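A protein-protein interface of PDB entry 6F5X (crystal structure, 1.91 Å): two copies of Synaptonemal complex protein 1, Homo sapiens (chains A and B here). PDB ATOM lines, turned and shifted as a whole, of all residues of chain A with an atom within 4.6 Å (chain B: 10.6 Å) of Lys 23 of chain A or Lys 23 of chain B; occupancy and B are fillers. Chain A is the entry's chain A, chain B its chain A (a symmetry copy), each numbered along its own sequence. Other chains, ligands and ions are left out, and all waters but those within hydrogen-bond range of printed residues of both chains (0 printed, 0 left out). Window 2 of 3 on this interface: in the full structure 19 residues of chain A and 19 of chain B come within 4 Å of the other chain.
NZ of Lys 23 of chain A sits close to NZ of Lys 23 of chain B (2.7 Å).
The side-chain hydroxyl (OG1) of Thr 26 of chain A is in hydrogen-bond range of the backbone carbonyl oxygen (O) of Trp 22 of chain A, at 3.1 Å.
O of Lys 23 of chain A lies within hydrogen-bond range of OG1 of Thr 26 of chain A (3.2 Å).
OG1 of Thr 26 of chain B is in hydrogen-bond range of O of Trp 22 of chain B, 3.1 Å away.
O of Lys 23 of chain B is in hydrogen-bond range of OG1 of Thr 26 of chain B.
Among the printed residues, merely in contact across the chains: Ile 19 of chain A with Ile 19 of chain B (3.7 Å), Trp 22 of chain A with Trp 22 of chain B (3.1 Å), Trp 22 of chain A with Lys 23 of chain B (3.2 Å), Trp 22 of chain A with Thr 26 of chain B (3.2 Å), Lys 23 of chain A with Trp 22 of chain B (3.2 Å) and Thr 26 of chain A with Trp 22 of chain B (3.2 Å).
Ile 19 of chain A touches just one residue of chain B: Ile 19.
Trp 22 of chain A touches just these residues of chain B: Trp 22 (3.1 Å), Lys 23 (3.2 Å) and Thr 26 (3.2 Å).
Of chain B, only Trp 22 and Lys 23 come within 4 Å of Lys 23 of chain A.
No residue of chain B comes within 4 Å of Ser 25 of chain A.
Thr 26 of chain A touches one residue of chain B.
No residue of chain B comes within 4 Å of Glu 27 of chain A.
Of the printed residues of chain A, Ile 19 of chain B touches Ile 19.
Printed residues of chain A within 4 Å of Trp 22 of chain B: Trp 22, Lys 23 and Thr 26.
Lys 23 of chain B touches just these residues of chain A: Trp 22 (3.2 Å) and Lys 23 (2.7 Å).
Printed residues of chain A within 4 Å of Thr 26 of chain B: Trp 22 (3.2 Å).
The nearest residue of chain B that does not touch Lys 23 of chain A is Ile 19 of chain B (4.5 Å).
The nearest residue of chain A that does not touch Lys 23 of chain B is Ile 19 of chain A (4.5 Å).
Hydrophobic or aromatic side chains of chain A within 4 Å of the printed part of chain B: Ile 19 and Trp 22.
Of the 17 printed residues of chain B, 4 touch a printed residue of chain A.
Printed residues of chain B that touch a printed residue of chain A: Ile 19, Trp 22, Lys 23 and Thr 26.
Hydrophobic or aromatic side chains of chain B within 4 Å of the printed part of chain A: Ile 19 and Trp 22.
Among the printed residues, 7 pairs touch across the chains.
Ile 19 of chain A touches its own counterpart, Ile 19 of chain B.
Trp 22 of chain A touches its own counterpart, Trp 22 of chain B.
Trp 22 of chain A touches Lys 23 of chain B, and with the chains exchanged Lys 23 of chain A touches Trp 22 of chain B.
Lys 23 of chain B touches its own counterpart, Lys 23 of chain A.
Of the 7 pairs that touch across the chains among the printed residues, 7 have their exchanged pair printed and touching as well.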
ATOM      1  N   ILE A  19     -10.581   6.458  -6.676  1.00  0.00           N
ATOM      2  CA  ILE A  19      -9.912   6.562  -7.967  1.00  0.00           C
ATOM      3  C   ILE A  19     -10.812   6.050  -9.080  1.00  0.00           C
ATOM      4  O   ILE A  19     -10.952   6.699 -10.116  1.00  0.00           O
ATOM      5  CB  ILE A  19      -8.565   5.828  -7.918  1.00  0.00           C
ATOM      6  CG1 ILE A  19      -7.622   6.599  -6.985  1.00  0.00           C
ATOM      7  CG2 ILE A  19      -8.010   5.624  -9.308  1.00  0.00           C
ATOM      8  CD1 ILE A  19      -6.368   5.861  -6.611  1.00  0.00           C
ATOM      9  N   LYS A  20     -11.462   4.902  -8.874  1.00  0.00           N
ATOM     10  CA  LYS A  20     -12.439   4.424  -9.847  1.00  0.00           C
ATOM     11  C   LYS A  20     -13.503   5.479 -10.131  1.00  0.00           C
ATOM     12  O   LYS A  20     -13.814   5.778 -11.292  1.00  0.00           O
ATOM     13  CB  LYS A  20     -13.094   3.137  -9.348  1.00  0.00           C
ATOM     14  CG  LYS A  20     -14.102   2.554 -10.337  1.00  0.00           C
ATOM     15  CD  LYS A  20     -14.725   1.246  -9.850  1.00  0.00           C
ATOM     16  CE  LYS A  20     -15.741   0.698 -10.856  1.00  0.00           C
ATOM     17  NZ  LYS A  20     -16.348  -0.584 -10.386  1.00  0.00           N
ATOM     18  N   LYS A  21     -14.090   6.039  -9.069  1.00  0.00           N
ATOM     19  CA  LYS A  21     -15.080   7.097  -9.232  1.00  0.00           C
ATOM     20  C   LYS A  21     -14.510   8.267 -10.021  1.00  0.00           C
ATOM     21  O   LYS A  21     -15.191   8.837 -10.885  1.00  0.00           O
ATOM     22  CB  LYS A  21     -15.570   7.568  -7.861  1.00  0.00           C
ATOM     23  CG  LYS A  21     -16.651   8.647  -7.892  1.00  0.00           C
ATOM     24  CD  LYS A  21     -17.123   8.983  -6.464  1.00  0.00           C
ATOM     25  CE  LYS A  21     -18.210  10.059  -6.438  1.00  0.00           C
ATOM     26  NZ  LYS A  21     -18.683  10.369  -5.051  1.00  0.00           N
ATOM     27  N   TRP A  22     -13.257   8.636  -9.749  1.00  0.00           N
ATOM     28  CA  TRP A  22     -12.671   9.736 -10.503  1.00  0.00           C
ATOM     29  C   TRP A  22     -12.582   9.365 -11.978  1.00  0.00           C
ATOM     30  O   TRP A  22     -12.847  10.194 -12.852  1.00  0.00           O
ATOM     31  CB  TRP A  22     -11.278  10.085  -9.975  1.00  0.00           C
ATOM     32  CG  TRP A  22     -10.794  11.476 -10.401  1.00  0.00           C
ATOM     33  CD1 TRP A  22     -11.218  12.665  -9.880  1.00  0.00           C
ATOM     34  CD2 TRP A  22      -9.893  11.817 -11.472  1.00  0.00           C
ATOM     35  NE1 TRP A  22     -10.598  13.716 -10.507  1.00  0.00           N
ATOM     36  CE2 TRP A  22      -9.787  13.227 -11.493  1.00  0.00           C
ATOM     37  CE3 TRP A  22      -9.161  11.077 -12.398  1.00  0.00           C
ATOM     38  CZ2 TRP A  22      -8.976  13.908 -12.406  1.00  0.00           C
ATOM     39  CZ3 TRP A  22      -8.359  11.764 -13.310  1.00  0.00           C
ATOM     40  CH2 TRP A  22      -8.272  13.160 -13.303  1.00  0.00           C
ATOM     41  N   LYS A  23     -12.203   8.119 -12.270  1.00  0.00           N
ATOM     42  CA  LYS A  23     -12.088   7.674 -13.655  1.00  0.00           C
ATOM     43  C   LYS A  23     -13.405   7.834 -14.380  1.00  0.00           C
ATOM     44  O   LYS A  23     -13.475   8.459 -15.446  1.00  0.00           O
ATOM     45  CB  LYS A  23     -11.650   6.212 -13.704  1.00  0.00           C
ATOM     46  CG  LYS A  23     -10.335   5.987 -13.033  1.00  0.00           C
ATOM     47  CD  LYS A  23      -9.252   6.645 -13.817  1.00  0.00           C
ATOM     48  CE  LYS A  23      -7.927   6.474 -13.151  1.00  0.00           C
ATOM     49  NZ  LYS A  23      -7.981   7.304 -11.935  1.00  0.00           N
ATOM     50  N   VAL A  24     -14.462   7.245 -13.818  1.00  0.00           N
ATOM     51  CA  VAL A  24     -15.795   7.386 -14.398  1.00  0.00           C
ATOM     52  C   VAL A  24     -16.096   8.853 -14.677  1.00  0.00           C
ATOM     53  O   VAL A  24     -16.446   9.236 -15.804  1.00  0.00           O
ATOM     54  CB  VAL A  24     -16.842   6.756 -13.464  1.00  0.00           C
ATOM     55  CG1 VAL A  24     -18.253   7.052 -13.937  1.00  0.00           C
ATOM     56  CG2 VAL A  24     -16.611   5.262 -13.387  1.00  0.00           C
ATOM     57  N   SER A  25     -15.914   9.699 -13.658  1.00  0.00           N
ATOM     58  CA  SER A  25     -16.252  11.115 -13.783  1.00  0.00           C
ATOM     59  C   SER A  25     -15.480  11.782 -14.927  1.00  0.00           C
ATOM     60  O   SER A  25     -16.075  12.424 -15.806  1.00  0.00           O
ATOM     61  CB  SER A  25     -15.985  11.809 -12.449  1.00  0.00           C
ATOM     62  OG  SER A  25     -16.259  13.191 -12.518  1.00  0.00           O
ATOM     63  N   THR A  26     -14.153  11.619 -14.949  1.00  0.00           N
ATOM     64  CA  THR A  26     -13.334  12.361 -15.901  1.00  0.00           C
ATOM     65  C   THR A  26     -13.530  11.853 -17.319  1.00  0.00           C
ATOM     66  O   THR A  26     -13.558  12.647 -18.265  1.00  0.00           O
ATOM     67  CB  THR A  26     -11.865  12.285 -15.513  1.00  0.00           C
ATOM     68  OG1 THR A  26     -11.443  10.920 -15.517  1.00  0.00           O
ATOM     69  CG2 THR A  26     -11.694  12.841 -14.147  1.00  0.00           C
ATOM     70  N   GLU A  27     -13.662  10.538 -17.492  1.00  0.00           N
ATOM     71  CA  GLU A  27     -13.963  10.015 -18.820  1.00  0.00           C
ATOM     72  C   GLU A  27     -15.291  10.558 -19.328  1.00  0.00           C
ATOM     73  O   GLU A  27     -15.374  11.053 -20.456  1.00  0.00           O
ATOM     74  CB  GLU A  27     -13.972   8.487 -18.804  1.00  0.00           C
ATOM     75  CG  GLU A  27     -12.601   7.880 -18.612  1.00  0.00           C
ATOM     76  CD  GLU A  27     -12.638   6.369 -18.604  1.00  0.00           C
ATOM     77  OE1 GLU A  27     -13.752   5.803 -18.614  1.00  0.00           O
ATOM     78  OE2 GLU A  27     -11.554   5.748 -18.596  1.00  0.00           O
ATOM     79  N   GLU B  15       1.631   1.267  -9.029  1.00  0.00           N
ATOM     80  CA  GLU B  15       0.273   1.668  -9.380  1.00  0.00           C
ATOM     81  C   GLU B  15       0.029   3.135  -9.073  1.00  0.00           C
ATOM     82  O   GLU B  15      -0.615   3.837  -9.860  1.00  0.00           O
ATOM     83  CB  GLU B  15      -0.757   0.780  -8.675  1.00  0.00           C
ATOM     84  CG  GLU B  15      -0.707  -0.617  -9.232  1.00  0.00           C
ATOM     85  CD  GLU B  15      -1.058  -0.654 -10.715  1.00  0.00           C
ATOM     86  OE1 GLU B  15      -1.893   0.178 -11.149  1.00  0.00           O
ATOM     87  OE2 GLU B  15      -0.493  -1.507 -11.440  1.00  0.00           O
ATOM     88  N   ALA B  16       0.540   3.618  -7.946  1.00  0.00           N
ATOM     89  CA  ALA B  16       0.439   5.040  -7.646  1.00  0.00           C
ATOM     90  C   ALA B  16       1.100   5.877  -8.724  1.00  0.00           C
ATOM     91  O   ALA B  16       0.582   6.933  -9.108  1.00  0.00           O
ATOM     92  CB  ALA B  16       1.082   5.332  -6.299  1.00  0.00           C
ATOM     93  N   GLU B  17       2.262   5.442  -9.215  1.00  0.00           N
ATOM     94  CA  GLU B  17       2.885   6.196 -10.295  1.00  0.00           C
ATOM     95  C   GLU B  17       2.002   6.197 -11.544  1.00  0.00           C
ATOM     96  O   GLU B  17       1.855   7.229 -12.214  1.00  0.00           O
ATOM     97  CB  GLU B  17       4.275   5.623 -10.601  1.00  0.00           C
ATOM     98  CG  GLU B  17       5.075   6.457 -11.584  1.00  0.00           C
ATOM     99  CD  GLU B  17       6.473   5.911 -11.859  1.00  0.00           C
ATOM    100  OE1 GLU B  17       6.809   4.830 -11.334  1.00  0.00           O
ATOM    101  OE2 GLU B  17       7.244   6.585 -12.584  1.00  0.00           O
ATOM    102  N   LYS B  18       1.403   5.053 -11.882  1.00  0.00           N
ATOM    103  CA  LYS B  18       0.580   5.014 -13.088  1.00  0.00           C
ATOM    104  C   LYS B  18      -0.638   5.914 -12.939  1.00  0.00           C
ATOM    105  O   LYS B  18      -1.061   6.575 -13.900  1.00  0.00           O
ATOM    106  CB  LYS B  18       0.140   3.579 -13.396  1.00  0.00           C
ATOM    107  CG  LYS B  18       1.242   2.601 -13.805  1.00  0.00           C
ATOM    108  CD  LYS B  18       0.599   1.250 -14.092  1.00  0.00           C
ATOM    109  CE  LYS B  18       1.599   0.187 -14.456  1.00  0.00           C
ATOM    110  NZ  LYS B  18       0.920  -1.127 -14.684  1.00  0.00           N
ATOM    111  N   ILE B  19      -1.199   5.968 -11.735  1.00  0.00           N
ATOM    112  CA  ILE B  19      -2.393   6.772 -11.506  1.00  0.00           C
ATOM    113  C   ILE B  19      -2.054   8.254 -11.529  1.00  0.00           C
ATOM    114  O   ILE B  19      -2.746   9.041 -12.174  1.00  0.00           O
ATOM    115  CB  ILE B  19      -3.068   6.344 -10.196  1.00  0.00           C
ATOM    116  CG1 ILE B  19      -3.640   4.932 -10.379  1.00  0.00           C
ATOM    117  CG2 ILE B  19      -4.094   7.362  -9.759  1.00  0.00           C
ATOM    118  CD1 ILE B  19      -4.080   4.264  -9.107  1.00  0.00           C
ATOM    119  N   LYS B  20      -0.971   8.652 -10.858  1.00  0.00           N
ATOM    120  CA  LYS B  20      -0.519  10.037 -10.946  1.00  0.00           C
ATOM    121  C   LYS B  20      -0.312  10.464 -12.396  1.00  0.00           C
ATOM    122  O   LYS B  20      -0.787  11.524 -12.825  1.00  0.00           O
ATOM    123  CB  LYS B  20       0.775  10.221 -10.153  1.00  0.00           C
ATOM    124  CG  LYS B  20       1.287  11.661 -10.167  1.00  0.00           C
ATOM    125  CD  LYS B  20       2.559  11.846  -9.341  1.00  0.00           C
ATOM    126  CE  LYS B  20       3.055  13.295  -9.388  1.00  0.00           C
ATOM    127  NZ  LYS B  20       4.296  13.483  -8.577  1.00  0.00           N
ATOM    128  N   LYS B  21       0.422   9.650 -13.161  1.00  0.00           N
ATOM    129  CA  LYS B  21       0.632   9.939 -14.574  1.00  0.00           C
ATOM    130  C   LYS B  21      -0.693  10.073 -15.311  1.00  0.00           C
ATOM    131  O   LYS B  21      -0.856  10.963 -16.157  1.00  0.00           O
ATOM    132  CB  LYS B  21       1.486   8.840 -15.209  1.00  0.00           C
ATOM    133  CG  LYS B  21       1.822   9.048 -16.685  1.00  0.00           C
ATOM    134  CD  LYS B  21       2.749   7.927 -17.194  1.00  0.00           C
ATOM    135  CE  LYS B  21       3.119   8.089 -18.669  1.00  0.00           C
ATOM    136  NZ  LYS B  21       4.036   7.010 -19.157  1.00  0.00           N
ATOM    137  N   TRP B  22      -1.657   9.205 -14.999  1.00  0.00           N
ATOM    138  CA  TRP B  22      -2.946   9.320 -15.668  1.00  0.00           C
ATOM    139  C   TRP B  22      -3.593  10.655 -15.321  1.00  0.00           C
ATOM    140  O   TRP B  22      -4.187  11.309 -16.182  1.00  0.00           O
ATOM    141  CB  TRP B  22      -3.879   8.176 -15.265  1.00  0.00           C
ATOM    142  CG  TRP B  22      -5.051   7.975 -16.232  1.00  0.00           C
ATOM    143  CD1 TRP B  22      -4.980   7.396 -17.467  1.00  0.00           C
ATOM    144  CD2 TRP B  22      -6.412   8.427 -16.090  1.00  0.00           C
ATOM    145  NE1 TRP B  22      -6.211   7.398 -18.074  1.00  0.00           N
ATOM    146  CE2 TRP B  22      -7.106   8.032 -17.257  1.00  0.00           C
ATOM    147  CE3 TRP B  22      -7.110   9.108 -15.094  1.00  0.00           C
ATOM    148  CZ2 TRP B  22      -8.465   8.298 -17.452  1.00  0.00           C
ATOM    149  CZ3 TRP B  22      -8.464   9.375 -15.299  1.00  0.00           C
ATOM    150  CH2 TRP B  22      -9.123   8.968 -16.463  1.00  0.00           C
ATOM    151  N   LYS B  23      -3.491  11.071 -14.057  1.00  0.00           N
ATOM    152  CA  LYS B  23      -4.081  12.336 -13.631  1.00  0.00           C
ATOM    153  C   LYS B  23      -3.522  13.485 -14.440  1.00  0.00           C
ATOM    154  O   LYS B  23      -4.271  14.274 -15.029  1.00  0.00           O
ATOM    155  CB  LYS B  23      -3.810  12.571 -12.148  1.00  0.00           C
ATOM    156  CG  LYS B  23      -4.366  11.487 -11.286  1.00  0.00           C
ATOM    157  CD  LYS B  23      -5.856  11.530 -11.323  1.00  0.00           C
ATOM    158  CE  LYS B  23      -6.445  10.431 -10.502  1.00  0.00           C
ATOM    159  NZ  LYS B  23      -6.151   9.186 -11.232  1.00  0.00           N
ATOM    160  N   VAL B  24      -2.194  13.604 -14.452  1.00  0.00           N
ATOM    161  CA  VAL B  24      -1.542  14.640 -15.249  1.00  0.00           C
ATOM    162  C   VAL B  24      -2.082  14.628 -16.673  1.00  0.00           C
ATOM    163  O   VAL B  24      -2.547  15.654 -17.194  1.00  0.00           O
ATOM    164  CB  VAL B  24      -0.017  14.444 -15.216  1.00  0.00           C
ATOM    165  CG1 VAL B  24       0.682  15.380 -16.185  1.00  0.00           C
ATOM    166  CG2 VAL B  24       0.488  14.669 -13.807  1.00  0.00           C
ATOM    167  N   SER B  25      -2.071  13.447 -17.301  1.00  0.00           N
ATOM    168  CA  SER B  25      -2.486  13.332 -18.697  1.00  0.00           C
ATOM    169  C   SER B  25      -3.925  13.818 -18.902  1.00  0.00           C
ATOM    170  O   SER B  25      -4.192  14.665 -19.767  1.00  0.00           O
ATOM    171  CB  SER B  25      -2.315  11.882 -19.146  1.00  0.00           C
ATOM    172  OG  SER B  25      -2.735  11.699 -20.481  1.00  0.00           O
ATOM    173  N   THR B  26      -4.864  13.311 -18.096  1.00  0.00           N
ATOM    174  CA  THR B  26      -6.275  13.591 -18.341  1.00  0.00           C
ATOM    175  C   THR B  26      -6.620  15.034 -18.018  1.00  0.00           C
ATOM    176  O   THR B  26      -7.413  15.659 -18.731  1.00  0.00           O
ATOM    177  CB  THR B  26      -7.153  12.646 -17.534  1.00  0.00           C
ATOM    178  OG1 THR B  26      -6.888  12.825 -16.142  1.00  0.00           O
ATOM    179  CG2 THR B  26      -6.835  11.246 -17.912  1.00  0.00           C
ATOM    180  N   GLU B  27      -6.045  15.583 -16.948  1.00  0.00           N
ATOM    181  CA  GLU B  27      -6.259  16.998 -16.663  1.00  0.00           C
ATOM    182  C   GLU B  27      -5.748  17.864 -17.805  1.00  0.00           C
ATOM    183  O   GLU B  27      -6.462  18.747 -18.289  1.00  0.00           O
ATOM    184  CB  GLU B  27      -5.591  17.386 -15.346  1.00  0.00           C
ATOM    185  CG  GLU B  27      -6.266  16.791 -14.131  1.00  0.00           C
ATOM    186  CD  GLU B  27      -5.588  17.194 -12.842  1.00  0.00           C
ATOM    187  OE1 GLU B  27      -4.512  17.827 -12.910  1.00  0.00           O
ATOM    188  OE2 GLU B  27      -6.134  16.885 -11.762  1.00  0.00           O
ATOM    189  N   ALA B  28      -4.518  17.610 -18.262  1.00  0.00           N
ATOM    190  CA  ALA B  28      -3.965  18.382 -19.371  1.00  0.00           C
ATOM    191  C   ALA B  28      -4.885  18.338 -20.588  1.00  0.00           C
ATOM    192  O   ALA B  28      -5.156  19.371 -21.224  1.00  0.00           O
ATOM    193  CB  ALA B  28      -2.574  17.855 -19.720  1.00  0.00           C
ATOM    194  N   GLU B  29      -5.400  17.150 -20.916  1.00  0.00           N
ATOM    195  CA  GLU B  29      -6.298  17.084 -22.061  1.00  0.00           C
ATOM    196  C   GLU B  29      -7.591  17.841 -21.791  1.00  0.00           C
ATOM    197  O   GLU B  29      -8.151  18.467 -22.701  1.00  0.00           O
ATOM    198  CB  GLU B  29      -6.596  15.639 -22.443  1.00  0.00           C
ATOM    199  CG  GLU B  29      -7.415  15.546 -23.730  1.00  0.00           C
ATOM    200  CD  GLU B  29      -7.594  14.125 -24.217  1.00  0.00           C
ATOM    201  OE1 GLU B  29      -7.105  13.197 -23.535  1.00  0.00           O
ATOM    202  OE2 GLU B  29      -8.201  13.938 -25.292  1.00  0.00           O
ATOM    203  N   LEU B  30      -8.083  17.795 -20.553  1.00  0.00           N
ATOM    204  CA  LEU B  30      -9.271  18.573 -20.216  1.00  0.00           C
ATOM    205  C   LEU B  30      -9.044  20.061 -20.449  1.00  0.00           C
ATOM    206  O   LEU B  30      -9.880  20.735 -21.053  1.00  0.00           O
ATOM    207  CB  LEU B  30      -9.683  18.306 -18.770  1.00  0.00           C
ATOM    208  CG  LEU B  30     -10.316  16.945 -18.519  1.00  0.00           C
ATOM    209  CD1 LEU B  30     -10.513  16.708 -17.029  1.00  0.00           C
ATOM    210  CD2 LEU B  30     -11.653  16.941 -19.234  1.00  0.00           C
ATOM    211  N   ARG B  31      -7.920  20.592 -19.966  1.00  0.00           N
ATOM    212  CA  ARG B  31      -7.644  22.010 -20.153  1.00  0.00           C
ATOM    213  C   ARG B  31      -7.541  22.349 -21.624  1.00  0.00           C
ATOM    214  O   ARG B  31      -7.955  23.435 -22.044  1.00  0.00           O
ATOM    215  CB  ARG B  31      -6.359  22.415 -19.437  1.00  0.00           C
ATOM    216  CG  ARG B  31      -6.444  22.385 -17.926  1.00  0.00           C
ATOM    217  CD  ARG B  31      -5.107  22.762 -17.323  1.00  0.00           C
ATOM    218  NE  ARG B  31      -4.101  21.750 -17.625  1.00  0.00           N
ATOM    219  CZ  ARG B  31      -2.809  21.872 -17.350  1.00  0.00           C
ATOM    220  NH1 ARG B  31      -2.356  22.969 -16.758  1.00  0.00           N
ATOM    221  NH2 ARG B  31      -1.973  20.894 -17.669  1.00  0.00           N
